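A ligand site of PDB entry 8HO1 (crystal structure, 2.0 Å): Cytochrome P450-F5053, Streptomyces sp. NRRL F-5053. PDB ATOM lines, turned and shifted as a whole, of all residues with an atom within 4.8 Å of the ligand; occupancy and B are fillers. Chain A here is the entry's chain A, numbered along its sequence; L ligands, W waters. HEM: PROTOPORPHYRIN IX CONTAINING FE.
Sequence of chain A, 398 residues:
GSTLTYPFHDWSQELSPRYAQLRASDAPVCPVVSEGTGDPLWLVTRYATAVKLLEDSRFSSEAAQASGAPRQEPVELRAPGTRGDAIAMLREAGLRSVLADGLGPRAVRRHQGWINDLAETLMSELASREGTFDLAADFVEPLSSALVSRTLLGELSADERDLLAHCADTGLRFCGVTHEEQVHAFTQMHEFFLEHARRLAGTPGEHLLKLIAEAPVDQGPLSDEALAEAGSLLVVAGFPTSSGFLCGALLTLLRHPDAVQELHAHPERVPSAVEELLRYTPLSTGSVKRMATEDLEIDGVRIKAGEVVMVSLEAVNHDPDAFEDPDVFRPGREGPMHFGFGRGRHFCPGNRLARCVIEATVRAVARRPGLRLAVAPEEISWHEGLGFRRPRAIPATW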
ATOM      1  N   SER A  61      13.644  10.413 -14.771  1.00  0.00           N
ATOM      2  CA  SER A  61      14.810  11.197 -15.186  1.00  0.00           C
ATOM      3  C   SER A  61      15.965  10.281 -15.605  1.00  0.00           C
ATOM      4  O   SER A  61      16.635  10.524 -16.622  1.00  0.00           O
ATOM      5  CB  SER A  61      15.249  12.126 -14.060  1.00  0.00           C
ATOM      6  OG  SER A  61      16.524  12.680 -14.371  1.00  0.00           O
ATOM      7  N   ILE A  87      24.124  11.218  -9.542  1.00  0.00           N
ATOM      8  CA  ILE A  87      23.298  11.539  -8.390  1.00  0.00           C
ATOM      9  C   ILE A  87      22.535  10.311  -7.923  1.00  0.00           C
ATOM     10  O   ILE A  87      22.362  10.096  -6.717  1.00  0.00           O
ATOM     11  CB  ILE A  87      22.364  12.739  -8.705  1.00  0.00           C
ATOM     12  CG1 ILE A  87      21.777  13.357  -7.428  1.00  0.00           C
ATOM     13  CG2 ILE A  87      21.230  12.341  -9.663  1.00  0.00           C
ATOM     14  CD1 ILE A  87      22.815  13.821  -6.408  1.00  0.00           C
ATOM     15  N   ARG A  91      23.195   8.305  -4.449  1.00  0.00           N
ATOM     16  CA  ARG A  91      22.065   7.860  -3.658  1.00  0.00           C
ATOM     17  C   ARG A  91      22.035   6.332  -3.570  1.00  0.00           C
ATOM     18  O   ARG A  91      21.784   5.772  -2.496  1.00  0.00           O
ATOM     19  CB  ARG A  91      20.766   8.442  -4.237  1.00  0.00           C
ATOM     20  CG  ARG A  91      20.595   9.946  -3.932  1.00  0.00           C
ATOM     21  CD  ARG A  91      19.418  10.622  -4.661  1.00  0.00           C
ATOM     22  NE  ARG A  91      19.408  12.074  -4.467  1.00  0.00           N
ATOM     23  CZ  ARG A  91      18.871  12.950  -5.310  1.00  0.00           C
ATOM     24  NH1 ARG A  91      18.262  12.566  -6.419  1.00  0.00           N
ATOM     25  NH2 ARG A  91      18.941  14.254  -5.021  1.00  0.00           N
ATOM     26  N   LEU A 103      25.005  19.676   1.361  1.00  0.00           N
ATOM     27  CA  LEU A 103      24.251  20.656   0.600  1.00  0.00           C
ATOM     28  C   LEU A 103      23.150  21.353   1.380  1.00  0.00           C
ATOM     29  O   LEU A 103      22.628  22.367   0.896  1.00  0.00           O
ATOM     30  CB  LEU A 103      23.619  19.989  -0.635  1.00  0.00           C
ATOM     31  CG  LEU A 103      24.642  19.423  -1.610  1.00  0.00           C
ATOM     32  CD1 LEU A 103      23.924  18.632  -2.693  1.00  0.00           C
ATOM     33  CD2 LEU A 103      25.498  20.586  -2.175  1.00  0.00           C
ATOM     34  N   LEU A 147      32.319  29.513  -4.698  1.00  0.00           N
ATOM     35  CA  LEU A 147      31.253  28.600  -4.285  1.00  0.00           C
ATOM     36  C   LEU A 147      31.547  27.166  -4.722  1.00  0.00           C
ATOM     37  O   LEU A 147      31.412  26.218  -3.933  1.00  0.00           O
ATOM     38  CB  LEU A 147      29.915  29.056  -4.870  1.00  0.00           C
ATOM     39  CG  LEU A 147      28.709  28.142  -4.565  1.00  0.00           C
ATOM     40  CD1 LEU A 147      28.332  28.205  -3.110  1.00  0.00           C
ATOM     41  CD2 LEU A 147      27.507  28.469  -5.430  1.00  0.00           C
ATOM     42  N   LEU A 152      31.957  22.562  -3.048  1.00  0.00           N
ATOM     43  CA  LEU A 152      31.712  21.370  -3.867  1.00  0.00           C
ATOM     44  C   LEU A 152      32.968  20.550  -4.137  1.00  0.00           C
ATOM     45  O   LEU A 152      33.004  19.365  -3.796  1.00  0.00           O
ATOM     46  CB  LEU A 152      31.050  21.757  -5.195  1.00  0.00           C
ATOM     47  CG  LEU A 152      29.746  22.558  -5.130  1.00  0.00           C
ATOM     48  CD1 LEU A 152      29.236  22.840  -6.540  1.00  0.00           C
ATOM     49  CD2 LEU A 152      28.695  21.812  -4.294  1.00  0.00           C
ATOM     50  N   LEU A 233      29.609  15.574 -12.189  1.00  0.00           N
ATOM     51  CA  LEU A 233      28.239  15.977 -11.871  1.00  0.00           C
ATOM     52  C   LEU A 233      28.215  17.349 -11.197  1.00  0.00           C
ATOM     53  O   LEU A 233      27.411  18.216 -11.548  1.00  0.00           O
ATOM     54  CB  LEU A 233      27.579  14.929 -10.984  1.00  0.00           C
ATOM     55  CG  LEU A 233      26.294  15.387 -10.264  1.00  0.00           C
ATOM     56  CD1 LEU A 233      25.147  15.592 -11.237  1.00  0.00           C
ATOM     57  CD2 LEU A 233      25.884  14.432  -9.137  1.00  0.00           C
ATOM     58  N   LEU A 234      29.100  17.556 -10.217  1.00  0.00           N
ATOM     59  CA  LEU A 234      29.102  18.823  -9.508  1.00  0.00           C
ATOM     60  C   LEU A 234      29.518  19.973 -10.419  1.00  0.00           C
ATOM     61  O   LEU A 234      29.011  21.085 -10.271  1.00  0.00           O
ATOM     62  CB  LEU A 234      30.007  18.735  -8.284  1.00  0.00           C
ATOM     63  CG  LEU A 234      29.579  17.715  -7.223  1.00  0.00           C
ATOM     64  CD1 LEU A 234      30.618  17.568  -6.135  1.00  0.00           C
ATOM     65  CD2 LEU A 234      28.218  18.072  -6.614  1.00  0.00           C
ATOM     66  N   ALA A 237      26.396  20.609 -12.839  1.00  0.00           N
ATOM     67  CA  ALA A 237      25.203  21.041 -12.100  1.00  0.00           C
ATOM     68  C   ALA A 237      25.430  22.349 -11.360  1.00  0.00           C
ATOM     69  O   ALA A 237      24.464  23.078 -11.090  1.00  0.00           O
ATOM     70  CB  ALA A 237      24.791  19.961 -11.097  1.00  0.00           C
ATOM     71  N   GLY A 238      26.671  22.674 -10.998  1.00  0.00           N
ATOM     72  CA  GLY A 238      26.917  23.832 -10.171  1.00  0.00           C
ATOM     73  C   GLY A 238      27.569  25.027 -10.839  1.00  0.00           C
ATOM     74  O   GLY A 238      27.366  26.168 -10.409  1.00  0.00           O
ATOM     75  N   THR A 241      25.267  26.799 -14.160  1.00  0.00           N
ATOM     76  CA  THR A 241      24.010  27.239 -13.560  1.00  0.00           C
ATOM     77  C   THR A 241      24.231  28.462 -12.679  1.00  0.00           C
ATOM     78  O   THR A 241      23.568  29.481 -12.836  1.00  0.00           O
ATOM     79  CB  THR A 241      23.403  26.111 -12.720  1.00  0.00           C
ATOM     80  OG1 THR A 241      24.429  25.615 -11.867  1.00  0.00           O
ATOM     81  CG2 THR A 241      22.917  24.978 -13.622  1.00  0.00           C
ATOM     82  N   SER A 242      25.162  28.355 -11.714  1.00  0.00           N
ATOM     83  CA  SER A 242      25.417  29.458 -10.803  1.00  0.00           C
ATOM     84  C   SER A 242      25.896  30.690 -11.559  1.00  0.00           C
ATOM     85  O   SER A 242      25.422  31.800 -11.301  1.00  0.00           O
ATOM     86  CB  SER A 242      26.432  29.055  -9.733  1.00  0.00           C
ATOM     87  OG  SER A 242      25.921  27.993  -8.926  1.00  0.00           O
ATOM     88  N   PHE A 245      23.019  32.040 -13.753  1.00  0.00           N
ATOM     89  CA  PHE A 245      21.910  32.655 -13.030  1.00  0.00           C
ATOM     90  C   PHE A 245      22.334  33.957 -12.357  1.00  0.00           C
ATOM     91  O   PHE A 245      21.591  34.953 -12.390  1.00  0.00           O
ATOM     92  CB  PHE A 245      21.298  31.718 -11.979  1.00  0.00           C
ATOM     93  CG  PHE A 245      20.051  32.309 -11.369  1.00  0.00           C
ATOM     94  CD1 PHE A 245      18.846  32.255 -12.044  1.00  0.00           C
ATOM     95  CD2 PHE A 245      20.100  32.993 -10.171  1.00  0.00           C
ATOM     96  CE1 PHE A 245      17.690  32.838 -11.500  1.00  0.00           C
ATOM     97  CE2 PHE A 245      18.955  33.569  -9.608  1.00  0.00           C
ATOM     98  CZ  PHE A 245      17.753  33.491 -10.288  1.00  0.00           C
ATOM     99  N   LEU A 278      14.309  33.870  -9.168  1.00  0.00           N
ATOM    100  CA  LEU A 278      14.306  32.474  -9.599  1.00  0.00           C
ATOM    101  C   LEU A 278      13.137  32.148 -10.521  1.00  0.00           C
ATOM    102  O   LEU A 278      13.247  31.226 -11.356  1.00  0.00           O
ATOM    103  CB  LEU A 278      14.285  31.552  -8.375  1.00  0.00           C
ATOM    104  CG  LEU A 278      15.614  31.504  -7.613  1.00  0.00           C
ATOM    105  CD1 LEU A 278      15.459  30.996  -6.177  1.00  0.00           C
ATOM    106  CD2 LEU A 278      16.663  30.676  -8.383  1.00  0.00           C
ATOM    107  N   LEU A 283      17.116  30.942 -17.435  1.00  0.00           N
ATOM    108  CA  LEU A 283      18.427  30.315 -17.301  1.00  0.00           C
ATOM    109  C   LEU A 283      18.641  29.290 -18.405  1.00  0.00           C
ATOM    110  O   LEU A 283      19.342  29.571 -19.379  1.00  0.00           O
ATOM    111  CB  LEU A 283      18.594  29.671 -15.931  1.00  0.00           C
ATOM    112  CG  LEU A 283      19.957  28.989 -15.700  1.00  0.00           C
ATOM    113  CD1 LEU A 283      21.116  29.966 -15.917  1.00  0.00           C
ATOM    114  CD2 LEU A 283      20.030  28.368 -14.305  1.00  0.00           C
ATOM    115  N   VAL A 288      14.084  20.511 -18.851  1.00  0.00           N
ATOM    116  CA  VAL A 288      14.290  19.260 -18.119  1.00  0.00           C
ATOM    117  C   VAL A 288      13.564  18.137 -18.862  1.00  0.00           C
ATOM    118  O   VAL A 288      12.625  18.370 -19.626  1.00  0.00           O
ATOM    119  CB  VAL A 288      13.824  19.357 -16.660  1.00  0.00           C
ATOM    120  CG1 VAL A 288      14.504  20.515 -15.937  1.00  0.00           C
ATOM    121  CG2 VAL A 288      12.275  19.494 -16.556  1.00  0.00           C
ATOM    122  N   ARG A 290      12.068  13.842 -19.011  1.00  0.00           N
ATOM    123  CA  ARG A 290      11.657  12.594 -18.376  1.00  0.00           C
ATOM    124  C   ARG A 290      11.201  11.637 -19.458  1.00  0.00           C
ATOM    125  O   ARG A 290      10.658  12.045 -20.486  1.00  0.00           O
ATOM    126  CB  ARG A 290      10.534  12.814 -17.337  1.00  0.00           C
ATOM    127  CG  ARG A 290      10.814  13.870 -16.242  1.00  0.00           C
ATOM    128  CD  ARG A 290      11.809  13.387 -15.167  1.00  0.00           C
ATOM    129  NE  ARG A 290      11.945  14.348 -14.071  1.00  0.00           N
ATOM    130  CZ  ARG A 290      12.838  15.329 -14.015  1.00  0.00           C
ATOM    131  NH1 ARG A 290      13.681  15.551 -15.016  1.00  0.00           N
ATOM    132  NH2 ARG A 290      12.888  16.109 -12.940  1.00  0.00           N
ATOM    133  N   LEU A 313      11.224  25.070 -18.032  1.00  0.00           N
ATOM    134  CA  LEU A 313      10.982  25.751 -16.769  1.00  0.00           C
ATOM    135  C   LEU A 313      10.695  27.224 -17.003  1.00  0.00           C
ATOM    136  O   LEU A 313       9.862  27.826 -16.315  1.00  0.00           O
ATOM    137  CB  LEU A 313      12.188  25.587 -15.854  1.00  0.00           C
ATOM    138  CG  LEU A 313      12.628  24.138 -15.635  1.00  0.00           C
ATOM    139  CD1 LEU A 313      13.870  24.116 -14.776  1.00  0.00           C
ATOM    140  CD2 LEU A 313      11.518  23.301 -15.007  1.00  0.00           C
ATOM    141  N   PHE A 339       9.316  27.333 -10.671  1.00  0.00           N
ATOM    142  CA  PHE A 339      10.003  26.167 -11.207  1.00  0.00           C
ATOM    143  C   PHE A 339      11.494  26.393 -11.440  1.00  0.00           C
ATOM    144  O   PHE A 339      12.129  25.590 -12.135  1.00  0.00           O
ATOM    145  CB  PHE A 339       9.361  25.735 -12.530  1.00  0.00           C
ATOM    146  CG  PHE A 339       8.244  24.763 -12.373  1.00  0.00           C
ATOM    147  CD1 PHE A 339       7.097  25.107 -11.660  1.00  0.00           C
ATOM    148  CD2 PHE A 339       8.312  23.510 -12.956  1.00  0.00           C
ATOM    149  CE1 PHE A 339       6.039  24.219 -11.523  1.00  0.00           C
ATOM    150  CE2 PHE A 339       7.266  22.616 -12.823  1.00  0.00           C
ATOM    151  CZ  PHE A 339       6.136  22.973 -12.104  1.00  0.00           C
ATOM    152  N   GLY A 340      12.062  27.462 -10.884  1.00  0.00           N
ATOM    153  CA  GLY A 340      13.474  27.762 -11.116  1.00  0.00           C
ATOM    154  C   GLY A 340      14.387  26.633 -10.688  1.00  0.00           C
ATOM    155  O   GLY A 340      15.448  26.427 -11.291  1.00  0.00           O
ATOM    156  N   PHE A 341      13.995  25.878  -9.662  1.00  0.00           N
ATOM    157  CA  PHE A 341      14.748  24.726  -9.188  1.00  0.00           C
ATOM    158  C   PHE A 341      14.091  23.411  -9.591  1.00  0.00           C
ATOM    159  O   PHE A 341      14.456  22.351  -9.066  1.00  0.00           O
ATOM    160  CB  PHE A 341      14.914  24.767  -7.659  1.00  0.00           C
ATOM    161  CG  PHE A 341      15.855  25.853  -7.161  1.00  0.00           C
ATOM    162  CD1 PHE A 341      17.140  25.964  -7.641  1.00  0.00           C
ATOM    163  CD2 PHE A 341      15.435  26.754  -6.188  1.00  0.00           C
ATOM    164  CE1 PHE A 341      18.014  26.951  -7.182  1.00  0.00           C
ATOM    165  CE2 PHE A 341      16.283  27.743  -5.709  1.00  0.00           C
ATOM    166  CZ  PHE A 341      17.568  27.832  -6.207  1.00  0.00           C
ATOM    167  N   GLY A 342      13.099  23.455 -10.494  1.00  0.00           N
ATOM    168  CA  GLY A 342      12.404  22.236 -10.857  1.00  0.00           C
ATOM    169  C   GLY A 342      11.238  21.946  -9.921  1.00  0.00           C
ATOM    170  O   GLY A 342      10.639  22.839  -9.328  1.00  0.00           O
ATOM    171  N   ARG A 345      10.781  15.062  -6.989  1.00  0.00           N
ATOM    172  CA  ARG A 345      11.925  14.366  -6.389  1.00  0.00           C
ATOM    173  C   ARG A 345      13.259  14.943  -6.833  1.00  0.00           C
ATOM    174  O   ARG A 345      14.260  14.817  -6.115  1.00  0.00           O
ATOM    175  CB  ARG A 345      11.887  12.870  -6.748  1.00  0.00           C
ATOM    176  CG  ARG A 345      10.579  12.153  -6.422  1.00  0.00           C
ATOM    177  CD  ARG A 345      10.775  10.827  -5.679  1.00  0.00           C
ATOM    178  NE  ARG A 345      11.999  10.105  -5.998  1.00  0.00           N
ATOM    179  CZ  ARG A 345      12.748   9.456  -5.111  1.00  0.00           C
ATOM    180  NH1 ARG A 345      12.427   9.422  -3.825  1.00  0.00           N
ATOM    181  NH2 ARG A 345      13.861   8.852  -5.525  1.00  0.00           N
ATOM    182  N   HIS A 346      13.323  15.506  -8.042  1.00  0.00           N
ATOM    183  CA  HIS A 346      14.585  15.990  -8.575  1.00  0.00           C
ATOM    184  C   HIS A 346      14.746  17.491  -8.381  1.00  0.00           C
ATOM    185  O   HIS A 346      15.571  18.128  -9.062  1.00  0.00           O
ATOM    186  CB  HIS A 346      14.724  15.577 -10.039  1.00  0.00           C
ATOM    187  CG  HIS A 346      14.680  14.097 -10.232  1.00  0.00           C
ATOM    188  ND1 HIS A 346      15.723  13.276  -9.867  1.00  0.00           N
ATOM    189  CD2 HIS A 346      13.710  13.283 -10.719  1.00  0.00           C
ATOM    190  CE1 HIS A 346      15.400  12.020 -10.128  1.00  0.00           C
ATOM    191  NE2 HIS A 346      14.184  11.994 -10.642  1.00  0.00           N
ATOM    192  N   CYS A 348      16.201  20.747  -7.283  1.00  0.00           N
ATOM    193  CA  CYS A 348      17.637  20.970  -7.210  1.00  0.00           C
ATOM    194  C   CYS A 348      18.145  20.834  -5.774  1.00  0.00           C
ATOM    195  O   CYS A 348      17.797  21.649  -4.905  1.00  0.00           O
ATOM    196  CB  CYS A 348      18.004  22.358  -7.758  1.00  0.00           C
ATOM    197  SG  CYS A 348      19.752  22.796  -7.541  1.00  0.00           S
ATOM    198  N   PRO A 349      18.972  19.825  -5.497  1.00  0.00           N
ATOM    199  CA  PRO A 349      19.574  19.726  -4.156  1.00  0.00           C
ATOM    200  C   PRO A 349      20.593  20.809  -3.882  1.00  0.00           C
ATOM    201  O   PRO A 349      20.917  21.063  -2.703  1.00  0.00           O
ATOM    202  CB  PRO A 349      20.208  18.327  -4.155  1.00  0.00           C
ATOM    203  CG  PRO A 349      20.522  18.061  -5.603  1.00  0.00           C
ATOM    204  CD  PRO A 349      19.450  18.767  -6.408  1.00  0.00           C
ATOM    205  N   GLY A 350      21.093  21.477  -4.926  1.00  0.00           N
ATOM    206  CA  GLY A 350      21.876  22.687  -4.768  1.00  0.00           C
ATOM    207  C   GLY A 350      21.071  23.911  -4.387  1.00  0.00           C
ATOM    208  O   GLY A 350      21.657  24.987  -4.261  1.00  0.00           O
ATOM    209  N   LEU A 353      22.404  26.163  -1.204  1.00  0.00           N
ATOM    210  CA  LEU A 353      23.602  26.945  -1.487  1.00  0.00           C
ATOM    211  C   LEU A 353      23.359  27.981  -2.587  1.00  0.00           C
ATOM    212  O   LEU A 353      23.936  29.068  -2.560  1.00  0.00           O
ATOM    213  CB  LEU A 353      24.754  26.016  -1.871  1.00  0.00           C
ATOM    214  CG  LEU A 353      25.334  25.200  -0.718  1.00  0.00           C
ATOM    215  CD1 LEU A 353      26.243  24.088  -1.228  1.00  0.00           C
ATOM    216  CD2 LEU A 353      26.104  26.118   0.229  1.00  0.00           C
ATOM    217  N   ALA A 354      22.522  27.649  -3.585  1.00  0.00           N
ATOM    218  CA  ALA A 354      22.227  28.629  -4.632  1.00  0.00           C
ATOM    219  C   ALA A 354      21.481  29.823  -4.063  1.00  0.00           C
ATOM    220  O   ALA A 354      21.813  30.976  -4.352  1.00  0.00           O
ATOM    221  CB  ALA A 354      21.416  27.978  -5.758  1.00  0.00           C
HETATM  222  CHA HEM L   1      19.033  19.635 -10.499  1.00  0.00           C
HETATM  223  CHB HEM L   1      23.107  20.411  -8.011  1.00  0.00           C
HETATM  224  CHC HEM L   1      22.719  25.176  -8.705  1.00  0.00           C
HETATM  225  CHD HEM L   1      18.590  24.421 -11.089  1.00  0.00           C
HETATM  226  C1A HEM L   1      20.206  19.426  -9.834  1.00  0.00           C
HETATM  227  C2A HEM L   1      20.806  18.139  -9.563  1.00  0.00           C
HETATM  228  C3A HEM L   1      21.933  18.355  -8.871  1.00  0.00           C
HETATM  229  C4A HEM L   1      22.081  19.783  -8.681  1.00  0.00           C
HETATM  230  CMA HEM L   1      22.900  17.261  -8.376  1.00  0.00           C
HETATM  231  CAA HEM L   1      20.246  16.755  -9.992  1.00  0.00           C
HETATM  232  CBA HEM L   1      19.133  16.335  -9.025  1.00  0.00           C
HETATM  233  CGA HEM L   1      18.417  15.101  -9.511  1.00  0.00           C
HETATM  234  O1A HEM L   1      17.837  14.374  -8.658  1.00  0.00           O
HETATM  235  O2A HEM L   1      18.436  14.834 -10.746  1.00  0.00           O
HETATM  236  C1B HEM L   1      23.339  21.760  -7.956  1.00  0.00           C
HETATM  237  C2B HEM L   1      24.427  22.388  -7.241  1.00  0.00           C
HETATM  238  C3B HEM L   1      24.315  23.714  -7.445  1.00  0.00           C
HETATM  239  C4B HEM L   1      23.151  23.941  -8.270  1.00  0.00           C
HETATM  240  CMB HEM L   1      25.469  21.584  -6.432  1.00  0.00           C
HETATM  241  CAB HEM L   1      25.166  24.900  -6.924  1.00  0.00           C
HETATM  242  CBB HEM L   1      26.010  24.777  -5.898  1.00  0.00           C
HETATM  243  C1C HEM L   1      21.562  25.391  -9.409  1.00  0.00           C
HETATM  244  C2C HEM L   1      21.041  26.691  -9.813  1.00  0.00           C
HETATM  245  C3C HEM L   1      19.896  26.460 -10.489  1.00  0.00           C
HETATM  246  C4C HEM L   1      19.666  25.040 -10.506  1.00  0.00           C
HETATM  247  CMC HEM L   1      21.753  28.041  -9.526  1.00  0.00           C
HETATM  248  CAC HEM L   1      18.922  27.476 -11.121  1.00  0.00           C
HETATM  249  CBC HEM L   1      18.780  28.719 -10.656  1.00  0.00           C
HETATM  250  C1D HEM L   1      18.372  23.073 -11.103  1.00  0.00           C
HETATM  251  C2D HEM L   1      17.187  22.462 -11.653  1.00  0.00           C
HETATM  252  C3D HEM L   1      17.277  21.137 -11.496  1.00  0.00           C
HETATM  253  C4D HEM L   1      18.537  20.873 -10.831  1.00  0.00           C
HETATM  254  CMD HEM L   1      16.069  23.283 -12.310  1.00  0.00           C
HETATM  255  CAD HEM L   1      16.238  20.075 -11.924  1.00  0.00           C
HETATM  256  CBD HEM L   1      16.654  19.304 -13.167  1.00  0.00           C
HETATM  257  CGD HEM L   1      15.636  18.214 -13.509  1.00  0.00           C
HETATM  258  O1D HEM L   1      14.460  18.263 -13.062  1.00  0.00           O
HETATM  259  O2D HEM L   1      16.010  17.276 -14.258  1.00  0.00           O
HETATM  260  NA  HEM L   1      21.008  20.410  -9.286  1.00  0.00           N
HETATM  261  NB  HEM L   1      22.578  22.735  -8.570  1.00  0.00           N
HETATM  262  NC  HEM L   1      20.691  24.412  -9.845  1.00  0.00           N
HETATM  263  ND  HEM L   1      19.180  22.071 -10.607  1.00  0.00           N
HETATM  264 FE   HEM L   1      20.811  22.476  -9.501  1.00  0.00          FE
HETATM  265  O   HOH W   1      16.353  16.686 -16.843  1.00  0.00           O
HETATM  266  O   HOH W   2      22.087  22.353 -11.491  1.00  0.00           O
HETATM  267  O   HOH W   3      18.180  16.339 -13.444  1.00  0.00           O
HETATM  268  O   HOH W   4      12.995  18.975 -10.706  1.00  0.00           O
HETATM  269  O   HOH W   5      18.229  12.597 -12.022  1.00  0.00           O
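A ring nitrogen (ND1) of His 346 is in hydrogen-bond range of an oxygen (O1A) of the ligand, 2.7 Å away. NH2 of Arg 290 is in salt-bridge range of O1D of the ligand, 2.7 Å away. An iron atom (FE) of the ligand is bound by the side-chain sulfur (SG) of Cys 348 (2.3 Å). An oxygen (O1A) of the ligand is in salt-bridge range of the guanidinium group (NH1) of Arg 91, at 2.9 Å.
N of Cys 348 sits at hydrogen-bond distance from O of Phe 341. SG of Cys 348 sits close to N of Gly 350. OG1 of Thr 241 sits at hydrogen-bond distance from O of Gly 238 (3.3 Å). O of Ala 237 is in hydrogen-bond range of OG1 of Thr 241, at 2.7 Å. OG of Ser 242 is in hydrogen-bond range of O of Gly 238, 2.8 Å away.
NB of the ligand sits close to O of Ala 237, at 3.2 Å. CG2 of Ile 87 touches O2A of the ligand, at 3.9 Å. Leu 152 touches the ligand (CD1 to CBB, 3.8 Å). Gly 238 touches the ligand (CA to C3B, 3.8 Å). Thr 241 touches the ligand (OG1 to CHC, 3.6 Å). OG of Ser 242 touches CAB of the ligand, at 3.8 Å. Phe 245 touches the ligand (CD1 to CBC, 3.8 Å). Leu 278 touches the ligand (CD2 to CBC, 3.7 Å). Leu 283 touches the ligand. Val 288 touches the ligand (CG1 to CGD, 3.5 Å). Leu 313 touches the ligand. Gly 340 touches the ligand. Phe 341 touches the ligand. N of Gly 342 touches CMD of the ligand, 3.5 Å away. CD of Pro 349 touches C2A of the ligand, at 3.5 Å. CA of Gly 350 touches C2B of the ligand, 3.6 Å away. CB of Ala 354 touches CMC of the ligand, 3.8 Å away. The nearest printed residue that does not touch the ligand is Leu 233 (4.002 Å).
Water W5 lies within hydrogen-bond range of O2A of the ligand, OG of Ser 61 and ND1 of His 346. Water W1 lies within hydrogen-bond range of O2D of the ligand (2.7 Å) and NH1 of Arg 290 (3.4 Å). Water W4 lies within hydrogen-bond range of an oxygen (O1D) of the ligand (2.9 Å) and the backbone carbonyl oxygen (O) of His 346 (3.2 Å).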
